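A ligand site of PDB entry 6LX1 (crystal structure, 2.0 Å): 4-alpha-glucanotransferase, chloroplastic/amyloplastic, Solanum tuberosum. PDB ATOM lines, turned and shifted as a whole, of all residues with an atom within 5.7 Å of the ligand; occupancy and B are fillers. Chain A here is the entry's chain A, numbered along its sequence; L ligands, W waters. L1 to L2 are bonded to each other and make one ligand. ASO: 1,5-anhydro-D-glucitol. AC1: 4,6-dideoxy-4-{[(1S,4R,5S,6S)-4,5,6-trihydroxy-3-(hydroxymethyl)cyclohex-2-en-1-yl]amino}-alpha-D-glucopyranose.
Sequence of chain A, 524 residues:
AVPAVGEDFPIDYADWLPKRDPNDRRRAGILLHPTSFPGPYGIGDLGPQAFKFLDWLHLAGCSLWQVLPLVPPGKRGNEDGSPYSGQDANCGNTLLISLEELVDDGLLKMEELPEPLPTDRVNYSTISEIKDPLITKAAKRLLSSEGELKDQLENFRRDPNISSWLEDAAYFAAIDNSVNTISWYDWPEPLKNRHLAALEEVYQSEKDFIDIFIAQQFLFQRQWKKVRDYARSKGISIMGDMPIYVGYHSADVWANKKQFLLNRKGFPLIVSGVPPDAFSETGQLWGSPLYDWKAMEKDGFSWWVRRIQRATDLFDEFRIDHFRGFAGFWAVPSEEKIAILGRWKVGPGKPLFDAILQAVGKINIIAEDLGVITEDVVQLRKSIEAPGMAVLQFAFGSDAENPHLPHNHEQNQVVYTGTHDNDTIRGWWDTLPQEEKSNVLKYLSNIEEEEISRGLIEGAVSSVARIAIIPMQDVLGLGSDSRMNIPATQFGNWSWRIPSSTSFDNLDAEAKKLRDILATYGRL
Water W1 lies within hydrogen-bond range of the side-chain hydroxyl of Ser 82 (3.0 Å), an oxygen (O5) of AC1 L2 (3.1 Å) and the indole nitrogen of Trp 494 (3.2 Å).
OG of Ser 82 touches C6 of AC1 L2 (3.7 Å).
CB of Tyr 84 touches O5 of AC1 L2 (3.7 Å).
OG of Ser 85 touches C6 of AC1 L2, 2.9 Å away.
CA of Pro 487 touches O2 of AC1 L2, at 3.3 Å.
O of Thr 489 touches O2B of AC1 L2, at 3.9 Å.
CH2 of Trp 494 touches O3 of ASO L1, at 3.6 Å.
Hydrophobic or aromatic side chains within 4 Å of the ligand: Tyr 84, His 420, Pro 487 and Trp 494.
Within 4 Å of the ligand: Ser 82, Tyr 84, Ser 85, Arg 319, Asp 321, His 420, Asp 421, Asn 485, Pro 487, Ala 488, Thr 489, Gln 490 and Trp 494.
Along chain A the residues within 4 Å of the ligand span positions 82 to 494.
The nearest printed residue that does not touch the ligand is Trp 286 (4.4 Å).
NE2 of His 420 sits close to OH of Tyr 84.
The side-chain carboxylate (OD1) of Asp 421 lies close to a ring nitrogen (NE2) of His 420 (3.4 Å).
The guanidinium group (NH2) of Arg 319 lies within salt-bridge range of the side-chain carboxylate (OD2) of Asp 321, at 3.3 Å.
OH of Tyr 84 sits at hydrogen-bond distance from OD2 of Asp 241 (2.5 Å).
N of Tyr 84 sits close to OG of Ser 82, at 3.1 Å.
OG1 of Thr 489 lies within hydrogen-bond range of O of Ile 486 (2.9 Å).
OD1 of Asp 421 sits at hydrogen-bond distance from ND2 of Asn 485 (2.9 Å).
N of Asn 485 sits at hydrogen-bond distance from O of His 420, 3.1 Å away.
A ring nitrogen (NE2) of His 420 is in hydrogen-bond range of an oxygen (O2) of ASO L1, 2.9 Å away.
NE2 of Gln 490 lies within hydrogen-bond range of O2B of AC1 L2.
O2 of ASO L1 lies within hydrogen-bond range of NH2 of Arg 319.
The backbone NH (N) of Ala 488 sits at hydrogen-bond distance from an oxygen (O3) of AC1 L2, at 3.0 Å.
OD2 of Asp 321 is covalently linked to C1 of ASO L1, 1.4 Å away.
The side-chain amide nitrogen of Asn 485 is in hydrogen-bond range of an oxygen (O2) of AC1 L2.
The side-chain carboxylate (OD1) of Asp 421 is in hydrogen-bond range of an oxygen (O3) of ASO L1, 2.7 Å away.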
ATOM      1  N   SER A  82      12.780   1.846  -9.852  1.00  0.00           N
ATOM      2  CA  SER A  82      13.924   2.780 -10.037  1.00  0.00           C
ATOM      3  C   SER A  82      14.515   3.155  -8.687  1.00  0.00           C
ATOM      4  O   SER A  82      13.851   3.829  -7.896  1.00  0.00           O
ATOM      5  CB  SER A  82      13.559   4.040 -10.754  1.00  0.00           C
ATOM      6  OG  SER A  82      14.719   4.843 -10.852  1.00  0.00           O
ATOM      7  N   TYR A  84      16.465   5.538  -8.354  1.00  0.00           N
ATOM      8  CA  TYR A  84      16.692   7.007  -8.486  1.00  0.00           C
ATOM      9  C   TYR A  84      15.396   7.808  -8.371  1.00  0.00           C
ATOM     10  O   TYR A  84      15.527   9.018  -8.350  1.00  0.00           O
ATOM     11  CB  TYR A  84      17.493   7.308  -9.769  1.00  0.00           C
ATOM     12  CG  TYR A  84      18.872   6.685  -9.705  1.00  0.00           C
ATOM     13  CD1 TYR A  84      19.932   7.304  -9.091  1.00  0.00           C
ATOM     14  CD2 TYR A  84      19.083   5.417 -10.237  1.00  0.00           C
ATOM     15  CE1 TYR A  84      21.183   6.691  -9.009  1.00  0.00           C
ATOM     16  CE2 TYR A  84      20.319   4.788 -10.150  1.00  0.00           C
ATOM     17  CZ  TYR A  84      21.365   5.430  -9.518  1.00  0.00           C
ATOM     18  OH  TYR A  84      22.574   4.779  -9.468  1.00  0.00           O
ATOM     19  N   SER A  85      14.269   7.158  -8.127  1.00  0.00           N
ATOM     20  CA  SER A  85      12.924   7.753  -7.942  1.00  0.00           C
ATOM     21  C   SER A  85      12.407   7.324  -6.574  1.00  0.00           C
ATOM     22  O   SER A  85      11.330   6.753  -6.498  1.00  0.00           O
ATOM     23  CB  SER A  85      11.975   7.255  -9.038  1.00  0.00           C
ATOM     24  OG  SER A  85      12.472   7.669 -10.257  1.00  0.00           O
ATOM     25  N   ASP A 241      25.508   5.465  -3.713  1.00  0.00           N
ATOM     26  CA  ASP A 241      25.148   6.422  -4.772  1.00  0.00           C
ATOM     27  C   ASP A 241      23.959   7.224  -4.266  1.00  0.00           C
ATOM     28  O   ASP A 241      23.143   6.693  -3.520  1.00  0.00           O
ATOM     29  CB  ASP A 241      24.781   5.683  -6.060  1.00  0.00           C
ATOM     30  CG  ASP A 241      24.836   6.493  -7.336  1.00  0.00           C
ATOM     31  OD1 ASP A 241      25.207   7.715  -7.294  1.00  0.00           O
ATOM     32  OD2 ASP A 241      24.506   5.884  -8.398  1.00  0.00           O
ATOM     33  N   PRO A 243      21.142  10.478  -5.733  1.00  0.00           N
ATOM     34  CA  PRO A 243      20.795  11.536  -6.695  1.00  0.00           C
ATOM     35  C   PRO A 243      21.045  12.860  -5.953  1.00  0.00           C
ATOM     36  O   PRO A 243      20.770  12.932  -4.740  1.00  0.00           O
ATOM     37  CB  PRO A 243      19.329  11.221  -7.067  1.00  0.00           C
ATOM     38  CG  PRO A 243      18.796  10.432  -5.871  1.00  0.00           C
ATOM     39  CD  PRO A 243      19.977   9.673  -5.288  1.00  0.00           C
ATOM     40  N   GLN A 284      15.711  17.902 -21.358  1.00  0.00           N
ATOM     41  CA  GLN A 284      15.203  16.873 -20.391  1.00  0.00           C
ATOM     42  C   GLN A 284      14.587  17.588 -19.162  1.00  0.00           C
ATOM     43  O   GLN A 284      15.315  18.344 -18.451  1.00  0.00           O
ATOM     44  CB  GLN A 284      16.346  15.913 -20.072  1.00  0.00           C
ATOM     45  CG  GLN A 284      15.921  14.484 -19.732  1.00  0.00           C
ATOM     46  CD  GLN A 284      17.110  13.590 -19.450  1.00  0.00           C
ATOM     47  OE1 GLN A 284      18.253  13.920 -19.753  1.00  0.00           O
ATOM     48  NE2 GLN A 284      16.865  12.448 -18.825  1.00  0.00           N
ATOM     49  N   LEU A 285      13.274  17.425 -18.945  1.00  0.00           N
ATOM     50  CA  LEU A 285      12.543  17.932 -17.758  1.00  0.00           C
ATOM     51  C   LEU A 285      12.525  16.832 -16.695  1.00  0.00           C
ATOM     52  O   LEU A 285      11.726  15.911 -16.867  1.00  0.00           O
ATOM     53  CB  LEU A 285      11.114  18.332 -18.139  1.00  0.00           C
ATOM     54  CG  LEU A 285      10.257  18.851 -16.986  1.00  0.00           C
ATOM     55  CD1 LEU A 285      10.811  20.162 -16.453  1.00  0.00           C
ATOM     56  CD2 LEU A 285       8.803  19.029 -17.406  1.00  0.00           C
ATOM     57  N   TRP A 286      13.332  16.922 -15.645  1.00  0.00           N
ATOM     58  CA  TRP A 286      13.379  15.897 -14.565  1.00  0.00           C
ATOM     59  C   TRP A 286      12.279  16.149 -13.541  1.00  0.00           C
ATOM     60  O   TRP A 286      11.733  15.175 -13.087  1.00  0.00           O
ATOM     61  CB  TRP A 286      14.718  15.836 -13.854  1.00  0.00           C
ATOM     62  CG  TRP A 286      15.860  15.475 -14.736  1.00  0.00           C
ATOM     63  CD1 TRP A 286      15.823  14.788 -15.923  1.00  0.00           C
ATOM     64  CD2 TRP A 286      17.236  15.768 -14.466  1.00  0.00           C
ATOM     65  NE1 TRP A 286      17.097  14.661 -16.421  1.00  0.00           N
ATOM     66  CE2 TRP A 286      17.985  15.244 -15.549  1.00  0.00           C
ATOM     67  CE3 TRP A 286      17.894  16.437 -13.431  1.00  0.00           C
ATOM     68  CZ2 TRP A 286      19.363  15.374 -15.610  1.00  0.00           C
ATOM     69  CZ3 TRP A 286      19.264  16.556 -13.493  1.00  0.00           C
ATOM     70  CH2 TRP A 286      19.978  16.037 -14.582  1.00  0.00           C
ATOM     71  N   ARG A 319      29.012   7.926  -4.662  1.00  0.00           N
ATOM     72  CA  ARG A 319      28.859   8.829  -5.815  1.00  0.00           C
ATOM     73  C   ARG A 319      27.731   9.824  -5.524  1.00  0.00           C
ATOM     74  O   ARG A 319      26.752   9.448  -4.881  1.00  0.00           O
ATOM     75  CB  ARG A 319      28.546   8.006  -7.058  1.00  0.00           C
ATOM     76  CG  ARG A 319      28.657   8.791  -8.351  1.00  0.00           C
ATOM     77  CD  ARG A 319      28.367   7.867  -9.528  1.00  0.00           C
ATOM     78  NE  ARG A 319      26.933   7.726  -9.684  1.00  0.00           N
ATOM     79  CZ  ARG A 319      26.291   7.577 -10.852  1.00  0.00           C
ATOM     80  NH1 ARG A 319      26.966   7.474 -11.989  1.00  0.00           N
ATOM     81  NH2 ARG A 319      24.961   7.491 -10.898  1.00  0.00           N
ATOM     82  N   ASP A 321      25.195  11.664  -7.971  1.00  0.00           N
ATOM     83  CA  ASP A 321      24.723  11.774  -9.377  1.00  0.00           C
ATOM     84  C   ASP A 321      24.324  13.233  -9.648  1.00  0.00           C
ATOM     85  O   ASP A 321      23.608  13.829  -8.838  1.00  0.00           O
ATOM     86  CB  ASP A 321      23.623  10.736  -9.530  1.00  0.00           C
ATOM     87  CG  ASP A 321      23.121  10.434 -10.926  1.00  0.00           C
ATOM     88  OD1 ASP A 321      23.564  11.087 -11.865  1.00  0.00           O
ATOM     89  OD2 ASP A 321      22.346   9.429 -11.054  1.00  0.00           O
ATOM     90  N   GLU A 368      29.947  12.423 -10.029  1.00  0.00           N
ATOM     91  CA  GLU A 368      29.448  12.033 -11.377  1.00  0.00           C
ATOM     92  C   GLU A 368      29.547  13.302 -12.233  1.00  0.00           C
ATOM     93  O   GLU A 368      28.871  14.295 -11.920  1.00  0.00           O
ATOM     94  CB  GLU A 368      28.012  11.492 -11.341  1.00  0.00           C
ATOM     95  CG  GLU A 368      27.481  11.174 -12.733  1.00  0.00           C
ATOM     96  CD  GLU A 368      26.861  12.352 -13.509  1.00  0.00           C
ATOM     97  OE1 GLU A 368      25.873  12.959 -13.009  1.00  0.00           O
ATOM     98  OE2 GLU A 368      27.296  12.618 -14.667  1.00  0.00           O
ATOM     99  N   HIS A 420      25.653   1.240 -14.677  1.00  0.00           N
ATOM    100  CA  HIS A 420      24.280   0.688 -14.791  1.00  0.00           C
ATOM    101  C   HIS A 420      23.485   1.405 -15.905  1.00  0.00           C
ATOM    102  O   HIS A 420      22.468   0.830 -16.313  1.00  0.00           O
ATOM    103  CB  HIS A 420      23.555   0.807 -13.430  1.00  0.00           C
ATOM    104  CG  HIS A 420      23.464   2.217 -13.014  1.00  0.00           C
ATOM    105  ND1 HIS A 420      24.526   2.877 -12.405  1.00  0.00           N
ATOM    106  CD2 HIS A 420      22.485   3.127 -13.202  1.00  0.00           C
ATOM    107  CE1 HIS A 420      24.163   4.109 -12.203  1.00  0.00           C
ATOM    108  NE2 HIS A 420      22.961   4.307 -12.730  1.00  0.00           N
ATOM    109  N   ASP A 421      23.886   2.613 -16.319  1.00  0.00           N
ATOM    110  CA  ASP A 421      23.254   3.388 -17.425  1.00  0.00           C
ATOM    111  C   ASP A 421      23.775   2.955 -18.806  1.00  0.00           C
ATOM    112  O   ASP A 421      23.176   3.351 -19.846  1.00  0.00           O
ATOM    113  CB  ASP A 421      23.435   4.896 -17.215  1.00  0.00           C
ATOM    114  CG  ASP A 421      22.588   5.502 -16.092  1.00  0.00           C
ATOM    115  OD1 ASP A 421      21.531   4.913 -15.780  1.00  0.00           O
ATOM    116  OD2 ASP A 421      23.046   6.467 -15.457  1.00  0.00           O
ATOM    117  N   ASN A 485      19.800  -0.576 -16.983  1.00  0.00           N
ATOM    118  CA  ASN A 485      18.980   0.618 -17.291  1.00  0.00           C
ATOM    119  C   ASN A 485      19.295   1.099 -18.711  1.00  0.00           C
ATOM    120  O   ASN A 485      20.484   1.180 -19.069  1.00  0.00           O
ATOM    121  CB  ASN A 485      19.196   1.765 -16.304  1.00  0.00           C
ATOM    122  CG  ASN A 485      18.310   2.953 -16.539  1.00  0.00           C
ATOM    123  OD1 ASN A 485      17.093   2.786 -16.659  1.00  0.00           O
ATOM    124  ND2 ASN A 485      18.860   4.146 -16.573  1.00  0.00           N
ATOM    125  N   ILE A 486      18.253   1.455 -19.473  1.00  0.00           N
ATOM    126  CA  ILE A 486      18.378   2.310 -20.693  1.00  0.00           C
ATOM    127  C   ILE A 486      17.864   3.690 -20.323  1.00  0.00           C
ATOM    128  O   ILE A 486      16.671   3.883 -20.092  1.00  0.00           O
ATOM    129  CB  ILE A 486      17.622   1.703 -21.908  1.00  0.00           C
ATOM    130  CG1 ILE A 486      18.033   0.264 -22.186  1.00  0.00           C
ATOM    131  CG2 ILE A 486      17.832   2.613 -23.117  1.00  0.00           C
ATOM    132  CD1 ILE A 486      17.212  -0.471 -23.252  1.00  0.00           C
ATOM    133  N   PRO A 487      18.715   4.712 -20.168  1.00  0.00           N
ATOM    134  CA  PRO A 487      18.233   6.029 -19.765  1.00  0.00           C
ATOM    135  C   PRO A 487      17.020   6.581 -20.554  1.00  0.00           C
ATOM    136  O   PRO A 487      17.010   6.474 -21.756  1.00  0.00           O
ATOM    137  CB  PRO A 487      19.456   6.901 -19.985  1.00  0.00           C
ATOM    138  CG  PRO A 487      20.614   5.958 -19.689  1.00  0.00           C
ATOM    139  CD  PRO A 487      20.182   4.643 -20.280  1.00  0.00           C
ATOM    140  N   ALA A 488      16.036   7.080 -19.817  1.00  0.00           N
ATOM    141  CA  ALA A 488      14.733   7.640 -20.273  1.00  0.00           C
ATOM    142  C   ALA A 488      13.726   6.554 -20.674  1.00  0.00           C
ATOM    143  O   ALA A 488      12.551   6.919 -20.845  1.00  0.00           O
ATOM    144  CB  ALA A 488      14.941   8.660 -21.362  1.00  0.00           C
ATOM    145  N   THR A 489      14.064   5.273 -20.797  1.00  0.00           N
ATOM    146  CA  THR A 489      13.036   4.255 -21.172  1.00  0.00           C
ATOM    147  C   THR A 489      12.159   3.930 -19.957  1.00  0.00           C
ATOM    148  O   THR A 489      12.558   4.277 -18.817  1.00  0.00           O
ATOM    149  CB  THR A 489      13.653   2.985 -21.765  1.00  0.00           C
ATOM    150  OG1 THR A 489      14.359   2.253 -20.747  1.00  0.00           O
ATOM    151  CG2 THR A 489      14.529   3.333 -22.944  1.00  0.00           C
ATOM    152  N   GLN A 490      10.993   3.316 -20.169  1.00  0.00           N
ATOM    153  CA  GLN A 490      10.009   3.145 -19.073  1.00  0.00           C
ATOM    154  C   GLN A 490       9.914   1.678 -18.647  1.00  0.00           C
ATOM    155  O   GLN A 490       9.342   1.469 -17.612  1.00  0.00           O
ATOM    156  CB  GLN A 490       8.656   3.733 -19.484  1.00  0.00           C
ATOM    157  CG  GLN A 490       8.678   5.242 -19.604  1.00  0.00           C
ATOM    158  CD  GLN A 490       9.459   5.873 -18.468  1.00  0.00           C
ATOM    159  OE1 GLN A 490       8.943   6.056 -17.368  1.00  0.00           O
ATOM    160  NE2 GLN A 490      10.727   6.182 -18.727  1.00  0.00           N
ATOM    161  N   TRP A 494      16.071  -2.063 -14.254  1.00  0.00           N
ATOM    162  CA  TRP A 494      16.368  -2.392 -12.829  1.00  0.00           C
ATOM    163  C   TRP A 494      15.978  -3.817 -12.475  1.00  0.00           C
ATOM    164  O   TRP A 494      15.924  -4.093 -11.286  1.00  0.00           O
ATOM    165  CB  TRP A 494      15.629  -1.382 -11.934  1.00  0.00           C
ATOM    166  CG  TRP A 494      15.676   0.036 -12.409  1.00  0.00           C
ATOM    167  CD1 TRP A 494      14.638   0.797 -12.813  1.00  0.00           C
ATOM    168  CD2 TRP A 494      16.844   0.868 -12.529  1.00  0.00           C
ATOM    169  NE1 TRP A 494      15.059   2.031 -13.197  1.00  0.00           N
ATOM    170  CE2 TRP A 494      16.414   2.104 -13.035  1.00  0.00           C
ATOM    171  CE3 TRP A 494      18.204   0.682 -12.262  1.00  0.00           C
ATOM    172  CZ2 TRP A 494      17.301   3.163 -13.271  1.00  0.00           C
ATOM    173  CZ3 TRP A 494      19.076   1.733 -12.470  1.00  0.00           C
ATOM    174  CH2 TRP A 494      18.623   2.972 -12.948  1.00  0.00           C
HETATM  175  C1  ASO L   1      21.644   9.273 -12.312  1.00  0.00           C
HETATM  176  C2  ASO L   1      21.465   7.790 -12.537  1.00  0.00           C
HETATM  177  C3  ASO L   1      20.428   7.535 -13.620  1.00  0.00           C
HETATM  178  C4  ASO L   1      19.114   8.239 -13.250  1.00  0.00           C
HETATM  179  C5  ASO L   1      19.401   9.694 -13.086  1.00  0.00           C
HETATM  180  C6  ASO L   1      18.108  10.471 -12.873  1.00  0.00           C
HETATM  181  O2  ASO L   1      22.709   7.175 -12.877  1.00  0.00           O
HETATM  182  O3  ASO L   1      20.214   6.144 -13.785  1.00  0.00           O
HETATM  183  O4  ASO L   1      18.201   8.117 -14.340  1.00  0.00           O
HETATM  184  O5  ASO L   1      20.359   9.874 -12.020  1.00  0.00           O
HETATM  185  O6  ASO L   1      18.375  11.610 -12.122  1.00  0.00           O
HETATM  186  C1  AC1 L   2      17.353   6.993 -14.251  1.00  0.00           C
HETATM  187  O2  AC1 L   2      17.788   6.907 -16.621  1.00  0.00           O
HETATM  188  C2  AC1 L   2      16.748   6.861 -15.637  1.00  0.00           C
HETATM  189  C4A AC1 L   2      10.010  10.168 -15.027  1.00  0.00           C
HETATM  190  C3  AC1 L   2      15.712   7.968 -15.899  1.00  0.00           C
HETATM  191  O3  AC1 L   2      15.021   7.484 -17.061  1.00  0.00           O
HETATM  192  C4  AC1 L   2      14.717   8.031 -14.729  1.00  0.00           C
HETATM  193  N4A AC1 L   2      13.546   8.836 -14.945  1.00  0.00           N
HETATM  194  C5  AC1 L   2      15.435   8.316 -13.425  1.00  0.00           C
HETATM  195  O5  AC1 L   2      16.346   7.191 -13.255  1.00  0.00           O
HETATM  196  C6  AC1 L   2      14.486   8.314 -12.205  1.00  0.00           C
HETATM  197  C1B AC1 L   2      12.208   8.206 -14.714  1.00  0.00           C
HETATM  198  C2B AC1 L   2      11.370   8.331 -15.976  1.00  0.00           C
HETATM  199  O2B AC1 L   2      12.110   7.729 -17.056  1.00  0.00           O
HETATM  200  C3B AC1 L   2      11.024   9.831 -16.104  1.00  0.00           C
HETATM  201  O3B AC1 L   2      10.440  10.199 -17.370  1.00  0.00           O
HETATM  202  O4  AC1 L   2       9.989  11.592 -14.973  1.00  0.00           O
HETATM  203  C5B AC1 L   2      10.332   9.531 -13.678  1.00  0.00           C
HETATM  204  C7B AC1 L   2      11.363   8.659 -13.539  1.00  0.00           C
HETATM  205  C6B AC1 L   2       9.432   9.800 -12.479  1.00  0.00           C
HETATM  206  O6B AC1 L   2       9.976  10.815 -11.630  1.00  0.00           O
HETATM  207  O   HOH W   1      14.082   5.082 -13.733  1.00  0.00           O
HETATM  208  O   HOH W   2      20.539  12.702 -10.199  1.00  0.00           O
HETATM  209  O   HOH W   3      19.044   9.185 -17.139  1.00  0.00           O
HETATM  210  O   HOH W   4      15.042  11.447 -15.058  1.00  0.00           O
HETATM  211  O   HOH W   5      14.975   4.318 -17.087  1.00  0.00           O
HETATM  212  O   HOH W   6      16.038  12.845 -11.922  1.00  0.00           O
